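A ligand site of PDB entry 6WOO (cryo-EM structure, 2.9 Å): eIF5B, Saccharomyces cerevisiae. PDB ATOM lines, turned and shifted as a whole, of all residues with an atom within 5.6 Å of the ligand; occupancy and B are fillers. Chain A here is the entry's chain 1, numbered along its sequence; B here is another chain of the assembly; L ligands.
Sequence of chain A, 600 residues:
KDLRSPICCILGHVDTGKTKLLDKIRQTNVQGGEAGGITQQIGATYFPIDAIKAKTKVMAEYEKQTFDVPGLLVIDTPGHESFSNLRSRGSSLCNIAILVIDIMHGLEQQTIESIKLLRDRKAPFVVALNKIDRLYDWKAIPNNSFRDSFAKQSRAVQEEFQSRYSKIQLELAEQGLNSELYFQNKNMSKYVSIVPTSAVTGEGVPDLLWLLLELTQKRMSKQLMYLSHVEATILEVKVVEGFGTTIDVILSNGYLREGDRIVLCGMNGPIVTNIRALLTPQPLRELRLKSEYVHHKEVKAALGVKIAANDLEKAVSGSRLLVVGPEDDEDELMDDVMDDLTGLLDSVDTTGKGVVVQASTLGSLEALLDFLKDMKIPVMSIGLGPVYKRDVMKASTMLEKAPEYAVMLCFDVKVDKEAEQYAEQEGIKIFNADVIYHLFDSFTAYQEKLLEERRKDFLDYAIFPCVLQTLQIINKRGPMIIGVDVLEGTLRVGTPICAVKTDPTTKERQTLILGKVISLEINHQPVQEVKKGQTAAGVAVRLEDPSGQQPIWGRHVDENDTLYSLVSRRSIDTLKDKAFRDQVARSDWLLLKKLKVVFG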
ATOM      1  N   HIS A  13     -12.538  -4.687   3.141  1.00  0.00           N
ATOM      2  CA  HIS A  13     -13.190  -5.154   4.397  1.00  0.00           C
ATOM      3  C   HIS A  13     -12.806  -4.189   5.513  1.00  0.00           C
ATOM      4  O   HIS A  13     -13.587  -3.251   5.774  1.00  0.00           O
ATOM      5  CB  HIS A  13     -12.869  -6.630   4.676  1.00  0.00           C
ATOM      6  CG  HIS A  13     -13.254  -7.059   6.049  1.00  0.00           C
ATOM      7  ND1 HIS A  13     -14.573  -7.180   6.435  1.00  0.00           N
ATOM      8  CD2 HIS A  13     -12.515  -7.375   7.133  1.00  0.00           C
ATOM      9  CE1 HIS A  13     -14.632  -7.557   7.701  1.00  0.00           C
ATOM     10  NE2 HIS A  13     -13.375  -7.681   8.146  1.00  0.00           N
ATOM     11  N   VAL A  14     -11.635  -4.393   6.126  1.00  0.00           N
ATOM     12  CA  VAL A  14     -11.085  -3.542   7.230  1.00  0.00           C
ATOM     13  C   VAL A  14      -9.547  -3.547   7.164  1.00  0.00           C
ATOM     14  O   VAL A  14      -8.964  -2.483   7.452  1.00  0.00           O
ATOM     15  CB  VAL A  14     -11.602  -3.993   8.610  1.00  0.00           C
ATOM     16  CG1 VAL A  14     -10.698  -3.544   9.763  1.00  0.00           C
ATOM     17  CG2 VAL A  14     -13.031  -3.509   8.853  1.00  0.00           C
ATOM     18  N   ASP A  15      -8.926  -4.699   6.873  1.00  0.00           N
ATOM     19  CA  ASP A  15      -7.443  -4.856   6.772  1.00  0.00           C
ATOM     20  C   ASP A  15      -7.084  -5.572   5.459  1.00  0.00           C
ATOM     21  O   ASP A  15      -6.019  -6.232   5.423  1.00  0.00           O
ATOM     22  CB  ASP A  15      -6.908  -5.572   8.008  1.00  0.00           C
ATOM     23  CG  ASP A  15      -6.475  -4.637   9.133  1.00  0.00           C
ATOM     24  OD1 ASP A  15      -7.249  -3.722   9.469  1.00  0.00           O
ATOM     25  OD2 ASP A  15      -5.371  -4.842   9.663  1.00  0.00           O
ATOM     26  N   THR A  16      -7.900  -5.421   4.416  1.00  0.00           N
ATOM     27  CA  THR A  16      -7.687  -6.071   3.098  1.00  0.00           C
ATOM     28  C   THR A  16      -6.416  -5.507   2.452  1.00  0.00           C
ATOM     29  O   THR A  16      -5.744  -6.277   1.751  1.00  0.00           O
ATOM     30  CB  THR A  16      -8.931  -5.919   2.198  1.00  0.00           C
ATOM     31  OG1 THR A  16      -9.505  -4.641   2.443  1.00  0.00           O
ATOM     32  CG2 THR A  16      -9.951  -7.012   2.459  1.00  0.00           C
ATOM     33  N   GLY A  17      -6.082  -4.240   2.706  1.00  0.00           N
ATOM     34  CA  GLY A  17      -4.945  -3.527   2.090  1.00  0.00           C
ATOM     35  C   GLY A  17      -5.430  -2.409   1.171  1.00  0.00           C
ATOM     36  O   GLY A  17      -4.971  -2.356   0.021  1.00  0.00           O
ATOM     37  N   LYS A  18      -6.310  -1.545   1.677  1.00  0.00           N
ATOM     38  CA  LYS A  18      -6.870  -0.372   0.956  1.00  0.00           C
ATOM     39  C   LYS A  18      -5.807   0.723   1.051  1.00  0.00           C
ATOM     40  O   LYS A  18      -5.347   1.207  -0.004  1.00  0.00           O
ATOM     41  CB  LYS A  18      -8.225   0.071   1.529  1.00  0.00           C
ATOM     42  CG  LYS A  18      -9.168  -1.040   1.981  1.00  0.00           C
ATOM     43  CD  LYS A  18     -10.181  -0.591   3.023  1.00  0.00           C
ATOM     44  CE  LYS A  18     -11.190   0.399   2.474  1.00  0.00           C
ATOM     45  NZ  LYS A  18     -12.558   0.168   3.007  1.00  0.00           N
ATOM     46  N   THR A  19      -5.403   1.033   2.280  1.00  0.00           N
ATOM     47  CA  THR A  19      -4.120   1.709   2.631  1.00  0.00           C
ATOM     48  C   THR A  19      -2.986   0.777   2.204  1.00  0.00           C
ATOM     49  O   THR A  19      -3.243  -0.415   1.978  1.00  0.00           O
ATOM     50  CB  THR A  19      -4.120   2.108   4.125  1.00  0.00           C
ATOM     51  OG1 THR A  19      -4.327   3.517   4.189  1.00  0.00           O
ATOM     52  CG2 THR A  19      -2.842   1.762   4.874  1.00  0.00           C
ATOM     53  N   LYS A  20      -1.779   1.320   2.049  1.00  0.00           N
ATOM     54  CA  LYS A  20      -0.528   0.591   1.703  1.00  0.00           C
ATOM     55  C   LYS A  20      -0.481   0.289   0.197  1.00  0.00           C
ATOM     56  O   LYS A  20       0.611   0.404  -0.387  1.00  0.00           O
ATOM     57  CB  LYS A  20      -0.356  -0.690   2.525  1.00  0.00           C
ATOM     58  CG  LYS A  20       1.061  -1.242   2.537  1.00  0.00           C
ATOM     59  CD  LYS A  20       1.295  -2.350   3.539  1.00  0.00           C
ATOM     60  CE  LYS A  20       2.765  -2.598   3.807  1.00  0.00           C
ATOM     61  NZ  LYS A  20       2.982  -3.277   5.104  1.00  0.00           N
ATOM     62  N   GLN A  31       2.158   5.094   4.870  1.00  0.00           N
ATOM     63  CA  GLN A  31       1.086   4.174   5.346  1.00  0.00           C
ATOM     64  C   GLN A  31       0.683   4.540   6.782  1.00  0.00           C
ATOM     65  O   GLN A  31      -0.525   4.527   7.070  1.00  0.00           O
ATOM     66  CB  GLN A  31       1.568   2.732   5.255  1.00  0.00           C
ATOM     67  CG  GLN A  31       0.503   1.672   5.540  1.00  0.00           C
ATOM     68  CD  GLN A  31       1.072   0.397   6.126  1.00  0.00           C
ATOM     69  OE1 GLN A  31       0.488  -0.205   7.015  1.00  0.00           O
ATOM     70  NE2 GLN A  31       2.220  -0.021   5.618  1.00  0.00           N
ATOM     71  N   GLY A  37      -2.457   1.735  12.631  1.00  0.00           N
ATOM     72  CA  GLY A  37      -2.756   1.021  11.370  1.00  0.00           C
ATOM     73  C   GLY A  37      -4.240   0.993  11.040  1.00  0.00           C
ATOM     74  O   GLY A  37      -4.671   0.014  10.392  1.00  0.00           O
ATOM     75  N   ILE A  38      -5.006   2.022  11.450  1.00  0.00           N
ATOM     76  CA  ILE A  38      -6.471   2.161  11.194  1.00  0.00           C
ATOM     77  C   ILE A  38      -6.742   3.543  10.578  1.00  0.00           C
ATOM     78  O   ILE A  38      -5.940   4.471  10.834  1.00  0.00           O
ATOM     79  CB  ILE A  38      -7.293   1.937  12.490  1.00  0.00           C
ATOM     80  CG1 ILE A  38      -7.056   3.012  13.550  1.00  0.00           C
ATOM     81  CG2 ILE A  38      -7.039   0.542  13.047  1.00  0.00           C
ATOM     82  CD1 ILE A  38      -8.326   3.647  14.070  1.00  0.00           C
ATOM     83  N   THR A  39      -7.816   3.681   9.806  1.00  0.00           N
ATOM     84  CA  THR A  39      -8.198   4.915   9.064  1.00  0.00           C
ATOM     85  C   THR A  39      -9.343   5.639   9.784  1.00  0.00           C
ATOM     86  O   THR A  39     -10.327   4.972  10.148  1.00  0.00           O
ATOM     87  CB  THR A  39      -8.610   4.608   7.625  1.00  0.00           C
ATOM     88  OG1 THR A  39      -7.434   4.207   6.930  1.00  0.00           O
ATOM     89  CG2 THR A  39      -9.264   5.773   6.909  1.00  0.00           C
ATOM     90  N   THR A  77      -8.611   6.023   1.843  1.00  0.00           N
ATOM     91  CA  THR A  77      -9.307   4.900   2.535  1.00  0.00           C
ATOM     92  C   THR A  77     -10.696   5.348   2.983  1.00  0.00           C
ATOM     93  O   THR A  77     -10.818   6.167   3.897  1.00  0.00           O
ATOM     94  CB  THR A  77      -8.469   4.386   3.706  1.00  0.00           C
ATOM     95  OG1 THR A  77      -7.185   4.007   3.207  1.00  0.00           O
ATOM     96  CG2 THR A  77      -9.092   3.198   4.419  1.00  0.00           C
ATOM     97  N   ASN A 130      -4.799  -8.637  -2.576  1.00  0.00           N
ATOM     98  CA  ASN A 130      -3.777  -7.714  -2.008  1.00  0.00           C
ATOM     99  C   ASN A 130      -2.521  -8.479  -1.574  1.00  0.00           C
ATOM    100  O   ASN A 130      -1.430  -8.037  -1.952  1.00  0.00           O
ATOM    101  CB  ASN A 130      -4.311  -6.915  -0.822  1.00  0.00           C
ATOM    102  CG  ASN A 130      -3.354  -5.833  -0.358  1.00  0.00           C
ATOM    103  OD1 ASN A 130      -3.212  -4.806  -1.008  1.00  0.00           O
ATOM    104  ND2 ASN A 130      -2.712  -6.061   0.768  1.00  0.00           N
ATOM    105  N   LYS A 131      -2.676  -9.525  -0.757  1.00  0.00           N
ATOM    106  CA  LYS A 131      -1.576 -10.111   0.064  1.00  0.00           C
ATOM    107  C   LYS A 131      -1.086 -11.422  -0.576  1.00  0.00           C
ATOM    108  O   LYS A 131      -1.087 -12.450   0.143  1.00  0.00           O
ATOM    109  CB  LYS A 131      -2.071 -10.289   1.503  1.00  0.00           C
ATOM    110  CG  LYS A 131      -2.677  -9.056   2.136  1.00  0.00           C
ATOM    111  CD  LYS A 131      -2.853  -9.166   3.642  1.00  0.00           C
ATOM    112  CE  LYS A 131      -3.531  -7.941   4.246  1.00  0.00           C
ATOM    113  NZ  LYS A 131      -3.810  -8.133   5.693  1.00  0.00           N
ATOM    114  N   ILE A 132      -0.646 -11.395  -1.837  1.00  0.00           N
ATOM    115  CA  ILE A 132      -0.148 -12.612  -2.561  1.00  0.00           C
ATOM    116  C   ILE A 132       1.324 -12.860  -2.198  1.00  0.00           C
ATOM    117  O   ILE A 132       1.822 -13.931  -2.571  1.00  0.00           O
ATOM    118  CB  ILE A 132      -0.363 -12.565  -4.087  1.00  0.00           C
ATOM    119  CG1 ILE A 132       0.797 -11.891  -4.844  1.00  0.00           C
ATOM    120  CG2 ILE A 132      -1.719 -11.967  -4.445  1.00  0.00           C
ATOM    121  CD1 ILE A 132       0.586 -11.759  -6.331  1.00  0.00           C
ATOM    122  N   ASP A 133       2.008 -11.945  -1.508  1.00  0.00           N
ATOM    123  CA  ASP A 133       3.370 -12.215  -0.985  1.00  0.00           C
ATOM    124  C   ASP A 133       3.284 -13.276   0.121  1.00  0.00           C
ATOM    125  O   ASP A 133       4.311 -13.934   0.378  1.00  0.00           O
ATOM    126  CB  ASP A 133       4.067 -10.927  -0.527  1.00  0.00           C
ATOM    127  CG  ASP A 133       3.649 -10.429   0.846  1.00  0.00           C
ATOM    128  OD1 ASP A 133       4.280 -10.841   1.842  1.00  0.00           O
ATOM    129  OD2 ASP A 133       2.687  -9.633   0.909  1.00  0.00           O
ATOM    130  N   ARG A 134       2.103 -13.426   0.752  1.00  0.00           N
ATOM    131  CA  ARG A 134       1.833 -14.409   1.834  1.00  0.00           C
ATOM    132  C   ARG A 134       1.373 -15.744   1.232  1.00  0.00           C
ATOM    133  O   ARG A 134       0.152 -15.975   1.154  1.00  0.00           O
ATOM    134  CB  ARG A 134       0.784 -13.848   2.808  1.00  0.00           C
ATOM    135  CG  ARG A 134       1.182 -12.520   3.433  1.00  0.00           C
ATOM    136  CD  ARG A 134       1.094 -12.511   4.946  1.00  0.00           C
ATOM    137  NE  ARG A 134      -0.277 -12.450   5.449  1.00  0.00           N
ATOM    138  CZ  ARG A 134      -0.959 -13.438   6.027  1.00  0.00           C
ATOM    139  NH1 ARG A 134      -2.207 -13.216   6.432  1.00  0.00           N
ATOM    140  NH2 ARG A 134      -0.425 -14.640   6.227  1.00  0.00           N
ATOM    141  N   THR A 197      -1.964  -8.450  -6.252  1.00  0.00           N
ATOM    142  CA  THR A 197      -1.140  -7.323  -5.734  1.00  0.00           C
ATOM    143  C   THR A 197      -0.144  -7.860  -4.698  1.00  0.00           C
ATOM    144  O   THR A 197      -0.268  -9.026  -4.328  1.00  0.00           O
ATOM    145  CB  THR A 197      -2.032  -6.255  -5.093  1.00  0.00           C
ATOM    146  OG1 THR A 197      -3.280  -6.203  -5.801  1.00  0.00           O
ATOM    147  CG2 THR A 197      -1.417  -4.874  -5.075  1.00  0.00           C
ATOM    148  N   SER A 198       0.792  -7.023  -4.256  1.00  0.00           N
ATOM    149  CA  SER A 198       1.539  -7.217  -2.983  1.00  0.00           C
ATOM    150  C   SER A 198       1.951  -5.846  -2.428  1.00  0.00           C
ATOM    151  O   SER A 198       3.094  -5.432  -2.669  1.00  0.00           O
ATOM    152  CB  SER A 198       2.719  -8.138  -3.153  1.00  0.00           C
ATOM    153  OG  SER A 198       3.605  -8.023  -2.040  1.00  0.00           O
ATOM    154  N   ALA A 199       1.054  -5.199  -1.695  1.00  0.00           N
ATOM    155  CA  ALA A 199       1.206  -3.816  -1.172  1.00  0.00           C
ATOM    156  C   ALA A 199       2.515  -3.670  -0.375  1.00  0.00           C
ATOM    157  O   ALA A 199       2.948  -2.508  -0.196  1.00  0.00           O
ATOM    158  CB  ALA A 199       0.005  -3.443  -0.359  1.00  0.00           C
ATOM    159  N   VAL A 200       3.124  -4.772   0.093  1.00  0.00           N
ATOM    160  CA  VAL A 200       4.476  -4.801   0.714  1.00  0.00           C
ATOM    161  C   VAL A 200       5.549  -4.629  -0.376  1.00  0.00           C
ATOM    162  O   VAL A 200       6.344  -3.674  -0.257  1.00  0.00           O
ATOM    163  CB  VAL A 200       4.692  -6.091   1.540  1.00  0.00           C
ATOM    164  CG1 VAL A 200       6.164  -6.413   1.774  1.00  0.00           C
ATOM    165  CG2 VAL A 200       3.956  -6.012   2.873  1.00  0.00           C
ATOM    166  P     G B2897       3.843  -7.391  11.252  1.00  0.00           P
ATOM    167  OP1   G B2897       3.040  -7.820  10.073  1.00  0.00           O
ATOM    168  OP2   G B2897       5.259  -7.005  11.065  1.00  0.00           O
ATOM    169  O5'   G B2897       3.092  -6.194  11.998  1.00  0.00           O
ATOM    170  C5'   G B2897       1.675  -5.920  11.810  1.00  0.00           C
ATOM    171  C4'   G B2897       0.807  -6.941  12.511  1.00  0.00           C
ATOM    172  O4'   G B2897       0.814  -6.695  13.949  1.00  0.00           O
ATOM    173  C3'   G B2897      -0.665  -6.945  12.094  1.00  0.00           C
ATOM    174  O3'   G B2897      -1.115  -8.298  11.933  1.00  0.00           O
ATOM    175  C2'   G B2897      -1.351  -6.250  13.268  1.00  0.00           C
ATOM    176  O2'   G B2897      -2.731  -6.526  13.396  1.00  0.00           O
ATOM    177  C1'   G B2897      -0.509  -6.771  14.428  1.00  0.00           C
ATOM    178  N9    G B2897      -0.616  -6.031  15.681  1.00  0.00           N
ATOM    179  C8    G B2897      -0.648  -4.667  15.834  1.00  0.00           C
ATOM    180  N7    G B2897      -0.740  -4.287  17.076  1.00  0.00           N
ATOM    181  C5    G B2897      -0.773  -5.477  17.797  1.00  0.00           C
ATOM    182  C6    G B2897      -0.867  -5.704  19.195  1.00  0.00           C
ATOM    183  O6    G B2897      -0.952  -4.880  20.111  1.00  0.00           O
ATOM    184  N1    G B2897      -0.867  -7.058  19.494  1.00  0.00           N
ATOM    185  C2    G B2897      -0.788  -8.078  18.567  1.00  0.00           C
ATOM    186  N2    G B2897      -0.790  -9.325  19.042  1.00  0.00           N
ATOM    187  N3    G B2897      -0.698  -7.879  17.252  1.00  0.00           N
ATOM    188  C4    G B2897      -0.696  -6.564  16.942  1.00  0.00           C
ATOM    189  P     U B2898      -2.420  -8.640  11.061  1.00  0.00           P
ATOM    190  OP1   U B2898      -2.366  -7.848   9.806  1.00  0.00           O
ATOM    191  OP2   U B2898      -3.605  -8.541  11.950  1.00  0.00           O
ATOM    192  O5'   U B2898      -2.199 -10.176  10.691  1.00  0.00           O
ATOM    193  C5'   U B2898      -1.231 -10.557   9.696  1.00  0.00           C
ATOM    194  C4'   U B2898      -0.706 -11.960   9.947  1.00  0.00           C
ATOM    195  O4'   U B2898       0.358 -11.929  10.925  1.00  0.00           O
ATOM    196  C3'   U B2898      -1.698 -12.987  10.478  1.00  0.00           C
ATOM    197  O3'   U B2898      -2.425 -13.544   9.400  1.00  0.00           O
ATOM    198  C2'   U B2898      -0.764 -13.993  11.120  1.00  0.00           C
ATOM    199  O2'   U B2898      -0.118 -14.850  10.203  1.00  0.00           O
ATOM    200  C1'   U B2898       0.256 -13.065  11.770  1.00  0.00           C
ATOM    201  N1    U B2898      -0.070 -12.615  13.135  1.00  0.00           N
ATOM    202  C2    U B2898      -0.052 -13.564  14.147  1.00  0.00           C
ATOM    203  O2    U B2898       0.219 -14.733  13.953  1.00  0.00           O
ATOM    204  N3    U B2898      -0.360 -13.074  15.394  1.00  0.00           N
ATOM    205  C4    U B2898      -0.673 -11.781  15.732  1.00  0.00           C
ATOM    206  O4    U B2898      -0.925 -11.498  16.904  1.00  0.00           O
ATOM    207  C5    U B2898      -0.665 -10.857  14.633  1.00  0.00           C
ATOM    208  C6    U B2898      -0.377 -11.300  13.404  1.00  0.00           C
HETATM  209  P1  LIG L   1      -7.225  -0.826   5.368  1.00  0.00           P
HETATM  210  O1  LIG L   1      -8.047  -1.979   4.823  1.00  0.00           O
HETATM  211  O2  LIG L   1      -6.547  -0.045   4.284  1.00  0.00           O
HETATM  212  O3  LIG L   1      -7.889   0.039   6.411  1.00  0.00           O
HETATM  213  O4  LIG L   1      -6.082  -1.615   6.166  1.00  0.00           O
HETATM  214  P2  LIG L   1      -4.513  -1.332   5.983  1.00  0.00           P
HETATM  215  O5  LIG L   1      -4.145  -1.382   4.526  1.00  0.00           O
HETATM  216  O6  LIG L   1      -4.180  -0.142   6.833  1.00  0.00           O
HETATM  217  O7  LIG L   1      -3.854  -2.626   6.646  1.00  0.00           O
HETATM  218  C1  LIG L   1      -2.462  -2.579   6.924  1.00  0.00           C
HETATM  219  C2  LIG L   1      -2.019  -3.864   7.615  1.00  0.00           C
HETATM  220  O8  LIG L   1      -2.232  -4.983   6.759  1.00  0.00           O
HETATM  221  C3  LIG L   1      -0.537  -3.796   7.956  1.00  0.00           C
HETATM  222  O9  LIG L   1      -0.321  -4.231   9.310  1.00  0.00           O
HETATM  223  C4  LIG L   1       0.143  -4.706   6.945  1.00  0.00           C
HETATM  224  O10 LIG L   1       1.153  -5.531   7.554  1.00  0.00           O
HETATM  225  C5  LIG L   1      -0.979  -5.547   6.354  1.00  0.00           C
HETATM  226  N1  LIG L   1      -0.860  -5.570   4.877  1.00  0.00           N
HETATM  227  C6  LIG L   1      -1.465  -4.727   4.011  1.00  0.00           C
HETATM  228  N2  LIG L   1      -1.132  -5.053   2.741  1.00  0.00           N
HETATM  229  C7  LIG L   1      -0.312  -6.109   2.774  1.00  0.00           C
HETATM  230  C8  LIG L   1       0.403  -6.951   1.779  1.00  0.00           C
HETATM  231  O11 LIG L   1       0.307  -6.732   0.556  1.00  0.00           O
HETATM  232  N3  LIG L   1       1.160  -7.961   2.231  1.00  0.00           N
HETATM  233  C9  LIG L   1       1.285  -8.222   3.548  1.00  0.00           C
HETATM  234  N4  LIG L   1       2.061  -9.250   3.950  1.00  0.00           N
HETATM  235  N5  LIG L   1       0.660  -7.495   4.513  1.00  0.00           N
HETATM  236  C10 LIG L   1      -0.137  -6.449   4.187  1.00  0.00           C
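The backbone NH (N) of Thr 19 is in hydrogen-bond range of an oxygen (O2) of the ligand (2.5 Å). The backbone carbonyl oxygen (O) of Thr 19 lies close to an oxygen (O5) of the ligand (2.9 Å). A nitrogen (N3) of the ligand sits at hydrogen-bond distance from the side-chain carboxylate of Asp 133, at 2.6 Å. The side-chain amide nitrogen of Asn 130 sits at hydrogen-bond distance from a nitrogen (N2) of the ligand, at 2.7 Å. An oxygen (O11) of the ligand lies within hydrogen-bond range of the backbone NH (N) of Ala 199, 2.8 Å away. The backbone carbonyl oxygen of Val 14 lies close to an oxygen (O1) of the ligand (2.8 Å). N of Lys 18 sits at hydrogen-bond distance from O2 of the ligand (3.0 Å). O11 of the ligand sits at hydrogen-bond distance from N of Val 200, at 3.5 Å. The backbone NH (N) of Thr 16 sits at hydrogen-bond distance from an oxygen (O1) of the ligand, 3.5 Å away.
The side-chain carboxylate (OD2) of Asp 133 sits close to the side-chain hydroxyl (OG) of Ser 198. The backbone carbonyl oxygen of Gly 17 lies close to the side-chain amide oxygen of Asn 130 (3.2 Å). ND2 of Asn 130 sits close to O of Thr 16 (3.2 Å). The backbone carbonyl oxygen (O) of Asn 130 sits close to the backbone NH (N) of Ser 198, at 3.4 Å. O3' of U 2898 of chain B lies within hydrogen-bond range of the guanidinium group (NH1) of Arg 134, 3.0 Å away. OG1 of Thr 16 lies within hydrogen-bond range of N of His 13 (3.1 Å). The side-chain amino group of Lys 131 lies within hydrogen-bond range of the backbone carbonyl oxygen of Asp 15, 2.9 Å away. NZ of Lys 20 sits close to NE2 of Gln 31.
Residues that only touch the ligand: Asp 15, Gly 17, Lys 20, Gln 31, Gly 37, Thr 77, Lys 131, Arg 134, Ser 198 and G 2897 of chain B. Hydrophobic or aromatic side chains that line the ligand: Ala 199 and Val 200. Of the 24 residues printed, 18 come within 4 Å of the ligand. The nearest printed residue that does not touch the ligand is U 2898 of chain B (4.2 Å).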
